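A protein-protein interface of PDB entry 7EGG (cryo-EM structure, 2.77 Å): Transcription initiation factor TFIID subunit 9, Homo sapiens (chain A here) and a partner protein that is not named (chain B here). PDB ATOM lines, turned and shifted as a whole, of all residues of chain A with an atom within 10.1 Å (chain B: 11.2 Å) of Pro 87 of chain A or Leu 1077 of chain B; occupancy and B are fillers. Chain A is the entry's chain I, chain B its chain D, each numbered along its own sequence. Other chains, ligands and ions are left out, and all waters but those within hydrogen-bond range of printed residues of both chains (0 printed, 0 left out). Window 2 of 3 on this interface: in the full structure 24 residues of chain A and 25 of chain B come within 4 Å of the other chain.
Of the 19 printed residues of chain B, 4 touch a printed residue of chain A. Hydrophobic or aromatic side chains of chain B within 4 Å of the printed part of chain A: His 1075, Leu 1077, Tyr 1080 and Leu 1084. Of the 12 printed residues of chain A, 5 touch a printed residue of chain B. Hydrophobic or aromatic side chains of chain A within 4 Å of the printed part of chain B: Pro 87, Phe 91, Leu 92 and Ile 95. Along chain A the printed residues that touch a printed residue of chain B span positions 84 to 95. Among the printed residues, 8 pairs touch across the chains. Among the printed residues, no Asp or Glu carboxylate lies within 4 Å of a Lys or Arg side-chain nitrogen of the other chain.
Of the printed residues of chain B, Thr 84 of chain A touches His 1075 (3.4 Å). No residue of chain B comes within 4 Å of Ser 85 of chain A. No residue of chain B comes within 4 Å of Pro 86 of chain A. No residue of chain B comes within 4 Å of Pro 88 of chain A. No residue of chain B comes within 4 Å of Arg 89 of chain A. Printed residues of chain B within 4 Å of Leu 92 of chain A: Tyr 1080 (3.7 Å). Printed residues of chain A within 4 Å of His 1075 of chain B: Thr 84 (3.4 Å). No residue of chain A comes within 4 Å of Leu 1078 of chain B. Tyr 1080 of chain B touches four residues of chain A. Printed residues of chain A within 4 Å of Leu 1084 of chain B: Ile 95. The nearest residue of chain A that does not touch Leu 1077 of chain B is Pro 88 of chain A (4.2 Å). The nearest printed residue of chain B that does not touch Ile 95 of chain A is Lys 1081 of chain B (4.8 Å).
Among the printed residues, merely in contact across the chains: Thr 84 of chain A with His 1075 of chain B (3.4 Å), Pro 87 of chain A with Leu 1077 of chain B (3.7 Å), Pro 87 of chain A with Tyr 1080 of chain B (3.8 Å), Phe 91 of chain A with Leu 1077 of chain B (3.9 Å), Phe 91 of chain A with Tyr 1080 of chain B (3.7 Å), Leu 92 of chain A with Tyr 1080 of chain B (3.7 Å), Ile 95 of chain A with Tyr 1080 of chain B (3.7 Å) and Ile 95 of chain A with Leu 1084 of chain B (3.8 Å).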
ATOM      1  N   THR A  84      -2.850  13.354 -30.436  1.00  0.00           N
ATOM      2  CA  THR A  84      -3.024  13.937 -29.120  1.00  0.00           C
ATOM      3  C   THR A  84      -3.032  12.841 -28.058  1.00  0.00           C
ATOM      4  O   THR A  84      -2.805  11.661 -28.335  1.00  0.00           O
ATOM      5  CB  THR A  84      -4.304  14.770 -29.056  1.00  0.00           C
ATOM      6  OG1 THR A  84      -5.441  13.900 -28.991  1.00  0.00           O
ATOM      7  CG2 THR A  84      -4.415  15.674 -30.272  1.00  0.00           C
ATOM      8  N   SER A  85      -3.297  13.242 -26.822  1.00  0.00           N
ATOM      9  CA  SER A  85      -3.210  12.360 -25.670  1.00  0.00           C
ATOM     10  C   SER A  85      -4.270  12.791 -24.669  1.00  0.00           C
ATOM     11  O   SER A  85      -4.831  13.886 -24.793  1.00  0.00           O
ATOM     12  CB  SER A  85      -1.806  12.412 -25.050  1.00  0.00           C
ATOM     13  OG  SER A  85      -1.532  13.694 -24.516  1.00  0.00           O
ATOM     14  N   PRO A  86      -4.591  11.949 -23.687  1.00  0.00           N
ATOM     15  CA  PRO A  86      -5.432  12.393 -22.564  1.00  0.00           C
ATOM     16  C   PRO A  86      -4.763  13.496 -21.757  1.00  0.00           C
ATOM     17  O   PRO A  86      -3.547  13.712 -21.879  1.00  0.00           O
ATOM     18  CB  PRO A  86      -5.596  11.110 -21.737  1.00  0.00           C
ATOM     19  CG  PRO A  86      -5.555  10.041 -22.737  1.00  0.00           C
ATOM     20  CD  PRO A  86      -4.543  10.475 -23.759  1.00  0.00           C
ATOM     21  N   PRO A  87      -5.532  14.229 -20.940  1.00  0.00           N
ATOM     22  CA  PRO A  87      -4.938  15.307 -20.143  1.00  0.00           C
ATOM     23  C   PRO A  87      -3.964  14.770 -19.106  1.00  0.00           C
ATOM     24  O   PRO A  87      -4.103  13.628 -18.638  1.00  0.00           O
ATOM     25  CB  PRO A  87      -6.160  15.967 -19.475  1.00  0.00           C
ATOM     26  CG  PRO A  87      -7.302  15.047 -19.728  1.00  0.00           C
ATOM     27  CD  PRO A  87      -6.996  14.349 -20.989  1.00  0.00           C
ATOM     28  N   PRO A  88      -2.956  15.556 -18.728  1.00  0.00           N
ATOM     29  CA  PRO A  88      -1.900  15.045 -17.846  1.00  0.00           C
ATOM     30  C   PRO A  88      -2.333  15.018 -16.386  1.00  0.00           C
ATOM     31  O   PRO A  88      -3.370  15.557 -16.003  1.00  0.00           O
ATOM     32  CB  PRO A  88      -0.746  16.036 -18.056  1.00  0.00           C
ATOM     33  CG  PRO A  88      -1.163  16.917 -19.198  1.00  0.00           C
ATOM     34  CD  PRO A  88      -2.644  16.910 -19.208  1.00  0.00           C
ATOM     35  N   ARG A  89      -1.486  14.390 -15.564  1.00  0.00           N
ATOM     36  CA  ARG A  89      -1.845  14.121 -14.175  1.00  0.00           C
ATOM     37  C   ARG A  89      -1.837  15.378 -13.320  1.00  0.00           C
ATOM     38  O   ARG A  89      -2.609  15.472 -12.361  1.00  0.00           O
ATOM     39  CB  ARG A  89      -0.898  13.085 -13.575  1.00  0.00           C
ATOM     40  N   ASP A  90      -0.982  16.349 -13.637  1.00  0.00           N
ATOM     41  CA  ASP A  90      -0.997  17.601 -12.893  1.00  0.00           C
ATOM     42  C   ASP A  90      -2.170  18.485 -13.284  1.00  0.00           C
ATOM     43  O   ASP A  90      -2.520  19.399 -12.531  1.00  0.00           O
ATOM     44  CB  ASP A  90       0.321  18.352 -13.087  1.00  0.00           C
ATOM     45  CG  ASP A  90       0.817  18.306 -14.518  1.00  0.00           C
ATOM     46  OD1 ASP A  90       0.019  18.006 -15.428  1.00  0.00           O
ATOM     47  OD2 ASP A  90       2.016  18.574 -14.738  1.00  0.00           O
ATOM     48  N   PHE A  91      -2.774  18.239 -14.444  1.00  0.00           N
ATOM     49  CA  PHE A  91      -3.982  18.936 -14.858  1.00  0.00           C
ATOM     50  C   PHE A  91      -5.231  18.258 -14.311  1.00  0.00           C
ATOM     51  O   PHE A  91      -6.210  18.935 -13.983  1.00  0.00           O
ATOM     52  CB  PHE A  91      -4.042  19.010 -16.386  1.00  0.00           C
ATOM     53  CG  PHE A  91      -5.275  19.685 -16.918  1.00  0.00           C
ATOM     54  CD1 PHE A  91      -5.382  21.065 -16.909  1.00  0.00           C
ATOM     55  CD2 PHE A  91      -6.319  18.942 -17.448  1.00  0.00           C
ATOM     56  CE1 PHE A  91      -6.510  21.687 -17.401  1.00  0.00           C
ATOM     57  CE2 PHE A  91      -7.448  19.556 -17.939  1.00  0.00           C
ATOM     58  CZ  PHE A  91      -7.542  20.931 -17.916  1.00  0.00           C
ATOM     59  N   LEU A  92      -5.213  16.931 -14.208  1.00  0.00           N
ATOM     60  CA  LEU A  92      -6.370  16.214 -13.684  1.00  0.00           C
ATOM     61  C   LEU A  92      -6.494  16.377 -12.179  1.00  0.00           C
ATOM     62  O   LEU A  92      -7.611  16.404 -11.654  1.00  0.00           O
ATOM     63  CB  LEU A  92      -6.282  14.734 -14.044  1.00  0.00           C
ATOM     64  CG  LEU A  92      -6.442  14.419 -15.528  1.00  0.00           C
ATOM     65  CD1 LEU A  92      -6.296  12.933 -15.778  1.00  0.00           C
ATOM     66  CD2 LEU A  92      -7.771  14.942 -16.034  1.00  0.00           C
ATOM     67  N   LEU A  93      -5.371  16.490 -11.472  1.00  0.00           N
ATOM     68  CA  LEU A  93      -5.410  16.653 -10.028  1.00  0.00           C
ATOM     69  C   LEU A  93      -5.727  18.080  -9.612  1.00  0.00           C
ATOM     70  O   LEU A  93      -6.124  18.302  -8.464  1.00  0.00           O
ATOM     71  CB  LEU A  93      -4.078  16.216  -9.418  1.00  0.00           C
ATOM     72  CG  LEU A  93      -3.870  14.704  -9.315  1.00  0.00           C
ATOM     73  CD1 LEU A  93      -2.399  14.372  -9.179  1.00  0.00           C
ATOM     74  CD2 LEU A  93      -4.647  14.143  -8.142  1.00  0.00           C
ATOM     75  N   ASP A  94      -5.573  19.047 -10.515  1.00  0.00           N
ATOM     76  CA  ASP A  94      -5.930  20.422 -10.196  1.00  0.00           C
ATOM     77  C   ASP A  94      -7.422  20.659 -10.388  1.00  0.00           C
ATOM     78  O   ASP A  94      -8.051  21.350  -9.580  1.00  0.00           O
ATOM     79  CB  ASP A  94      -5.106  21.388 -11.053  1.00  0.00           C
ATOM     80  CG  ASP A  94      -5.303  22.848 -10.662  1.00  0.00           C
ATOM     81  OD1 ASP A  94      -6.342  23.447 -11.013  1.00  0.00           O
ATOM     82  OD2 ASP A  94      -4.405  23.403  -9.993  1.00  0.00           O
ATOM     83  N   ILE A  95      -8.006  20.100 -11.451  1.00  0.00           N
ATOM     84  CA  ILE A  95      -9.445  20.226 -11.644  1.00  0.00           C
ATOM     85  C   ILE A  95     -10.220  19.303 -10.719  1.00  0.00           C
ATOM     86  O   ILE A  95     -11.424  19.507 -10.528  1.00  0.00           O
ATOM     87  CB  ILE A  95      -9.850  19.951 -13.102  1.00  0.00           C
ATOM     88  CG1 ILE A  95      -9.534  18.509 -13.491  1.00  0.00           C
ATOM     89  CG2 ILE A  95      -9.149  20.917 -14.039  1.00  0.00           C
ATOM     90  CD1 ILE A  95     -10.258  18.038 -14.727  1.00  0.00           C
ATOM     91  N   LEU B1063     -20.739  27.239 -27.719  1.00  0.00           N
ATOM     92  CA  LEU B1063     -19.307  27.289 -27.976  1.00  0.00           C
ATOM     93  C   LEU B1063     -18.680  25.906 -27.868  1.00  0.00           C
ATOM     94  O   LEU B1063     -17.785  25.572 -28.649  1.00  0.00           O
ATOM     95  CB  LEU B1063     -18.638  28.263 -27.010  1.00  0.00           C
ATOM     96  CG  LEU B1063     -17.167  28.584 -27.260  1.00  0.00           C
ATOM     97  CD1 LEU B1063     -16.955  30.071 -27.208  1.00  0.00           C
ATOM     98  CD2 LEU B1063     -16.299  27.908 -26.228  1.00  0.00           C
ATOM     99  N   ILE B1064     -19.138  25.096 -26.909  1.00  0.00           N
ATOM    100  CA  ILE B1064     -18.627  23.738 -26.744  1.00  0.00           C
ATOM    101  C   ILE B1064     -19.026  22.869 -27.931  1.00  0.00           C
ATOM    102  O   ILE B1064     -18.238  22.041 -28.408  1.00  0.00           O
ATOM    103  CB  ILE B1064     -19.126  23.166 -25.401  1.00  0.00           C
ATOM    104  CG1 ILE B1064     -18.296  23.720 -24.247  1.00  0.00           C
ATOM    105  CG2 ILE B1064     -19.090  21.649 -25.358  1.00  0.00           C
ATOM    106  CD1 ILE B1064     -18.863  23.388 -22.901  1.00  0.00           C
ATOM    107  N   LEU B1067     -16.676  23.223 -30.770  1.00  0.00           N
ATOM    108  CA  LEU B1067     -15.300  22.840 -30.485  1.00  0.00           C
ATOM    109  C   LEU B1067     -15.040  21.357 -30.658  1.00  0.00           C
ATOM    110  O   LEU B1067     -13.984  20.978 -31.163  1.00  0.00           O
ATOM    111  CB  LEU B1067     -14.912  23.238 -29.059  1.00  0.00           C
ATOM    112  CG  LEU B1067     -14.640  24.709 -28.772  1.00  0.00           C
ATOM    113  CD1 LEU B1067     -13.984  24.847 -27.412  1.00  0.00           C
ATOM    114  CD2 LEU B1067     -13.804  25.339 -29.868  1.00  0.00           C
ATOM    115  N   GLU B1068     -15.974  20.500 -30.249  1.00  0.00           N
ATOM    116  CA  GLU B1068     -15.783  19.067 -30.411  1.00  0.00           C
ATOM    117  C   GLU B1068     -16.042  18.592 -31.834  1.00  0.00           C
ATOM    118  O   GLU B1068     -15.765  17.428 -32.137  1.00  0.00           O
ATOM    119  CB  GLU B1068     -16.681  18.300 -29.439  1.00  0.00           C
ATOM    120  CG  GLU B1068     -18.089  18.847 -29.322  1.00  0.00           C
ATOM    121  CD  GLU B1068     -18.848  18.231 -28.166  1.00  0.00           C
ATOM    122  OE1 GLU B1068     -18.193  17.712 -27.240  1.00  0.00           O
ATOM    123  OE2 GLU B1068     -20.096  18.261 -28.184  1.00  0.00           O
ATOM    124  N   ARG B1071     -11.558  19.780 -35.966  1.00  0.00           N
ATOM    125  CA  ARG B1071     -10.473  18.842 -35.687  1.00  0.00           C
ATOM    126  C   ARG B1071      -9.516  19.397 -34.643  1.00  0.00           C
ATOM    127  O   ARG B1071      -9.133  18.692 -33.702  1.00  0.00           O
ATOM    128  CB  ARG B1071      -9.718  18.510 -36.970  1.00  0.00           C
ATOM    129  CG  ARG B1071      -8.822  17.301 -36.833  1.00  0.00           C
ATOM    130  CD  ARG B1071      -7.826  17.205 -37.964  1.00  0.00           C
ATOM    131  NE  ARG B1071      -7.077  15.958 -37.895  1.00  0.00           N
ATOM    132  CZ  ARG B1071      -5.987  15.779 -37.156  1.00  0.00           C
ATOM    133  NH1 ARG B1071      -5.510  16.771 -36.419  1.00  0.00           N
ATOM    134  NH2 ARG B1071      -5.372  14.605 -37.156  1.00  0.00           N
ATOM    135  N   GLU B1072      -9.097  20.646 -34.807  1.00  0.00           N
ATOM    136  CA  GLU B1072      -8.456  21.356 -33.715  1.00  0.00           C
ATOM    137  C   GLU B1072      -9.470  21.588 -32.602  1.00  0.00           C
ATOM    138  O   GLU B1072     -10.677  21.686 -32.847  1.00  0.00           O
ATOM    139  CB  GLU B1072      -7.876  22.684 -34.203  1.00  0.00           C
ATOM    140  CG  GLU B1072      -8.913  23.690 -34.689  1.00  0.00           C
ATOM    141  CD  GLU B1072      -9.082  23.683 -36.194  1.00  0.00           C
ATOM    142  OE1 GLU B1072      -8.283  23.014 -36.883  1.00  0.00           O
ATOM    143  OE2 GLU B1072     -10.014  24.352 -36.688  1.00  0.00           O
ATOM    144  N   THR B1073      -8.969  21.622 -31.364  1.00  0.00           N
ATOM    145  CA  THR B1073      -9.746  21.802 -30.132  1.00  0.00           C
ATOM    146  C   THR B1073     -10.836  20.745 -29.935  1.00  0.00           C
ATOM    147  O   THR B1073     -11.814  20.997 -29.228  1.00  0.00           O
ATOM    148  CB  THR B1073     -10.366  23.206 -30.033  1.00  0.00           C
ATOM    149  OG1 THR B1073     -11.422  23.332 -30.989  1.00  0.00           O
ATOM    150  CG2 THR B1073      -9.317  24.282 -30.283  1.00  0.00           C
ATOM    151  N   SER B1074     -10.698  19.559 -30.529  1.00  0.00           N
ATOM    152  CA  SER B1074     -11.604  18.461 -30.214  1.00  0.00           C
ATOM    153  C   SER B1074     -11.086  17.630 -29.054  1.00  0.00           C
ATOM    154  O   SER B1074     -11.849  17.286 -28.148  1.00  0.00           O
ATOM    155  CB  SER B1074     -11.818  17.562 -31.433  1.00  0.00           C
ATOM    156  OG  SER B1074     -10.637  16.859 -31.765  1.00  0.00           O
ATOM    157  N   HIS B1075      -9.802  17.286 -29.076  1.00  0.00           N
ATOM    158  CA  HIS B1075      -9.122  16.694 -27.931  1.00  0.00           C
ATOM    159  C   HIS B1075      -8.109  17.726 -27.453  1.00  0.00           C
ATOM    160  O   HIS B1075      -6.926  17.672 -27.787  1.00  0.00           O
ATOM    161  CB  HIS B1075      -8.455  15.384 -28.301  1.00  0.00           C
ATOM    162  CG  HIS B1075      -9.416  14.289 -28.638  1.00  0.00           C
ATOM    163  ND1 HIS B1075      -9.062  13.202 -29.406  1.00  0.00           N
ATOM    164  CD2 HIS B1075     -10.716  14.111 -28.307  1.00  0.00           C
ATOM    165  CE1 HIS B1075     -10.104  12.402 -29.537  1.00  0.00           C
ATOM    166  NE2 HIS B1075     -11.120  12.930 -28.878  1.00  0.00           N
ATOM    167  N   SER B1076      -8.585  18.668 -26.644  1.00  0.00           N
ATOM    168  CA  SER B1076      -7.755  19.752 -26.153  1.00  0.00           C
ATOM    169  C   SER B1076      -8.111  20.030 -24.704  1.00  0.00           C
ATOM    170  O   SER B1076      -9.213  19.726 -24.244  1.00  0.00           O
ATOM    171  CB  SER B1076      -7.926  21.023 -26.989  1.00  0.00           C
ATOM    172  OG  SER B1076      -9.215  21.575 -26.812  1.00  0.00           O
ATOM    173  N   LEU B1077      -7.159  20.622 -23.986  1.00  0.00           N
ATOM    174  CA  LEU B1077      -7.372  20.965 -22.588  1.00  0.00           C
ATOM    175  C   LEU B1077      -8.281  22.170 -22.407  1.00  0.00           C
ATOM    176  O   LEU B1077      -8.707  22.435 -21.279  1.00  0.00           O
ATOM    177  CB  LEU B1077      -6.034  21.236 -21.897  1.00  0.00           C
ATOM    178  CG  LEU B1077      -4.916  20.214 -22.076  1.00  0.00           C
ATOM    179  CD1 LEU B1077      -3.727  20.600 -21.219  1.00  0.00           C
ATOM    180  CD2 LEU B1077      -5.396  18.825 -21.725  1.00  0.00           C
ATOM    181  N   LEU B1078      -8.579  22.907 -23.472  1.00  0.00           N
ATOM    182  CA  LEU B1078      -9.469  24.050 -23.360  1.00  0.00           C
ATOM    183  C   LEU B1078     -10.929  23.643 -23.495  1.00  0.00           C
ATOM    184  O   LEU B1078     -11.801  24.293 -22.910  1.00  0.00           O
ATOM    185  CB  LEU B1078      -9.094  25.100 -24.414  1.00  0.00           C
ATOM    186  CG  LEU B1078      -9.533  26.560 -24.246  1.00  0.00           C
ATOM    187  CD1 LEU B1078      -8.490  27.466 -24.873  1.00  0.00           C
ATOM    188  CD2 LEU B1078     -10.889  26.849 -24.853  1.00  0.00           C
ATOM    189  N   LEU B1079     -11.214  22.581 -24.249  1.00  0.00           N
ATOM    190  CA  LEU B1079     -12.560  22.019 -24.286  1.00  0.00           C
ATOM    191  C   LEU B1079     -12.817  21.112 -23.092  1.00  0.00           C
ATOM    192  O   LEU B1079     -13.942  21.070 -22.579  1.00  0.00           O
ATOM    193  CB  LEU B1079     -12.773  21.251 -25.594  1.00  0.00           C
ATOM    194  CG  LEU B1079     -14.063  20.444 -25.774  1.00  0.00           C
ATOM    195  CD1 LEU B1079     -15.270  21.356 -25.776  1.00  0.00           C
ATOM    196  CD2 LEU B1079     -14.015  19.625 -27.039  1.00  0.00           C
ATOM    197  N   TYR B1080     -11.787  20.399 -22.635  1.00  0.00           N
ATOM    198  CA  TYR B1080     -11.918  19.523 -21.477  1.00  0.00           C
ATOM    199  C   TYR B1080     -12.198  20.314 -20.206  1.00  0.00           C
ATOM    200  O   TYR B1080     -12.968  19.870 -19.348  1.00  0.00           O
ATOM    201  CB  TYR B1080     -10.648  18.693 -21.324  1.00  0.00           C
ATOM    202  CG  TYR B1080     -10.765  17.531 -20.375  1.00  0.00           C
ATOM    203  CD1 TYR B1080     -11.213  16.296 -20.814  1.00  0.00           C
ATOM    204  CD2 TYR B1080     -10.404  17.663 -19.042  1.00  0.00           C
ATOM    205  CE1 TYR B1080     -11.309  15.231 -19.951  1.00  0.00           C
ATOM    206  CE2 TYR B1080     -10.499  16.606 -18.173  1.00  0.00           C
ATOM    207  CZ  TYR B1080     -10.947  15.393 -18.631  1.00  0.00           C
ATOM    208  OH  TYR B1080     -11.041  14.338 -17.759  1.00  0.00           O
ATOM    209  N   LYS B1081     -11.579  21.486 -20.063  1.00  0.00           N
ATOM    210  CA  LYS B1081     -11.870  22.328 -18.912  1.00  0.00           C
ATOM    211  C   LYS B1081     -13.212  23.031 -19.068  1.00  0.00           C
ATOM    212  O   LYS B1081     -13.867  23.344 -18.070  1.00  0.00           O
ATOM    213  CB  LYS B1081     -10.743  23.341 -18.710  1.00  0.00           C
ATOM    214  CG  LYS B1081     -10.768  24.051 -17.367  1.00  0.00           C
ATOM    215  CD  LYS B1081      -9.627  25.039 -17.229  1.00  0.00           C
ATOM    216  CE  LYS B1081      -9.692  25.755 -15.891  1.00  0.00           C
ATOM    217  NZ  LYS B1081      -8.613  26.767 -15.746  1.00  0.00           N
ATOM    218  N   ALA B1082     -13.648  23.260 -20.311  1.00  0.00           N
ATOM    219  CA  ALA B1082     -14.921  23.928 -20.563  1.00  0.00           C
ATOM    220  C   ALA B1082     -16.119  23.070 -20.192  1.00  0.00           C
ATOM    221  O   ALA B1082     -17.216  23.603 -20.010  1.00  0.00           O
ATOM    222  CB  ALA B1082     -15.024  24.328 -22.030  1.00  0.00           C
ATOM    223  N   PHE B1083     -15.930  21.758 -20.063  1.00  0.00           N
ATOM    224  CA  PHE B1083     -16.978  20.870 -19.582  1.00  0.00           C
ATOM    225  C   PHE B1083     -17.277  21.057 -18.101  1.00  0.00           C
ATOM    226  O   PHE B1083     -18.282  20.522 -17.618  1.00  0.00           O
ATOM    227  CB  PHE B1083     -16.581  19.420 -19.843  1.00  0.00           C
ATOM    228  CG  PHE B1083     -16.846  18.968 -21.243  1.00  0.00           C
ATOM    229  CD1 PHE B1083     -18.017  19.322 -21.887  1.00  0.00           C
ATOM    230  CD2 PHE B1083     -15.922  18.192 -21.920  1.00  0.00           C
ATOM    231  CE1 PHE B1083     -18.265  18.903 -23.173  1.00  0.00           C
ATOM    232  CE2 PHE B1083     -16.166  17.775 -23.206  1.00  0.00           C
ATOM    233  CZ  PHE B1083     -17.338  18.131 -23.836  1.00  0.00           C
ATOM    234  N   LEU B1084     -16.435  21.791 -17.374  1.00  0.00           N
ATOM    235  CA  LEU B1084     -16.614  22.024 -15.953  1.00  0.00           C
ATOM    236  C   LEU B1084     -16.849  23.487 -15.612  1.00  0.00           C
ATOM    237  O   LEU B1084     -16.948  23.821 -14.426  1.00  0.00           O
ATOM    238  CB  LEU B1084     -15.393  21.505 -15.185  1.00  0.00           C
ATOM    239  CG  LEU B1084     -15.020  20.053 -15.480  1.00  0.00           C
ATOM    240  CD1 LEU B1084     -13.533  19.832 -15.320  1.00  0.00           C
ATOM    241  CD2 LEU B1084     -15.794  19.120 -14.579  1.00  0.00           C
ATOM    242  N   LYS B1085     -16.949  24.367 -16.605  1.00  0.00           N
ATOM    243  CA  LYS B1085     -17.158  25.790 -16.358  1.00  0.00           C
ATOM    244  C   LYS B1085     -18.635  26.153 -16.360  1.00  0.00           C
ATOM    245  O   LYS B1085     -18.993  27.328 -16.437  1.00  0.00           O
ATOM    246  CB  LYS B1085     -16.425  26.632 -17.401  1.00  0.00           C
ATOM    247  CG  LYS B1085     -14.923  26.661 -17.234  1.00  0.00           C
ATOM    248  CD  LYS B1085     -14.262  27.269 -18.453  1.00  0.00           C
ATOM    249  CE  LYS B1085     -12.757  27.108 -18.399  1.00  0.00           C
ATOM    250  NZ  LYS B1085     -12.140  27.306 -19.737  1.00  0.00           N
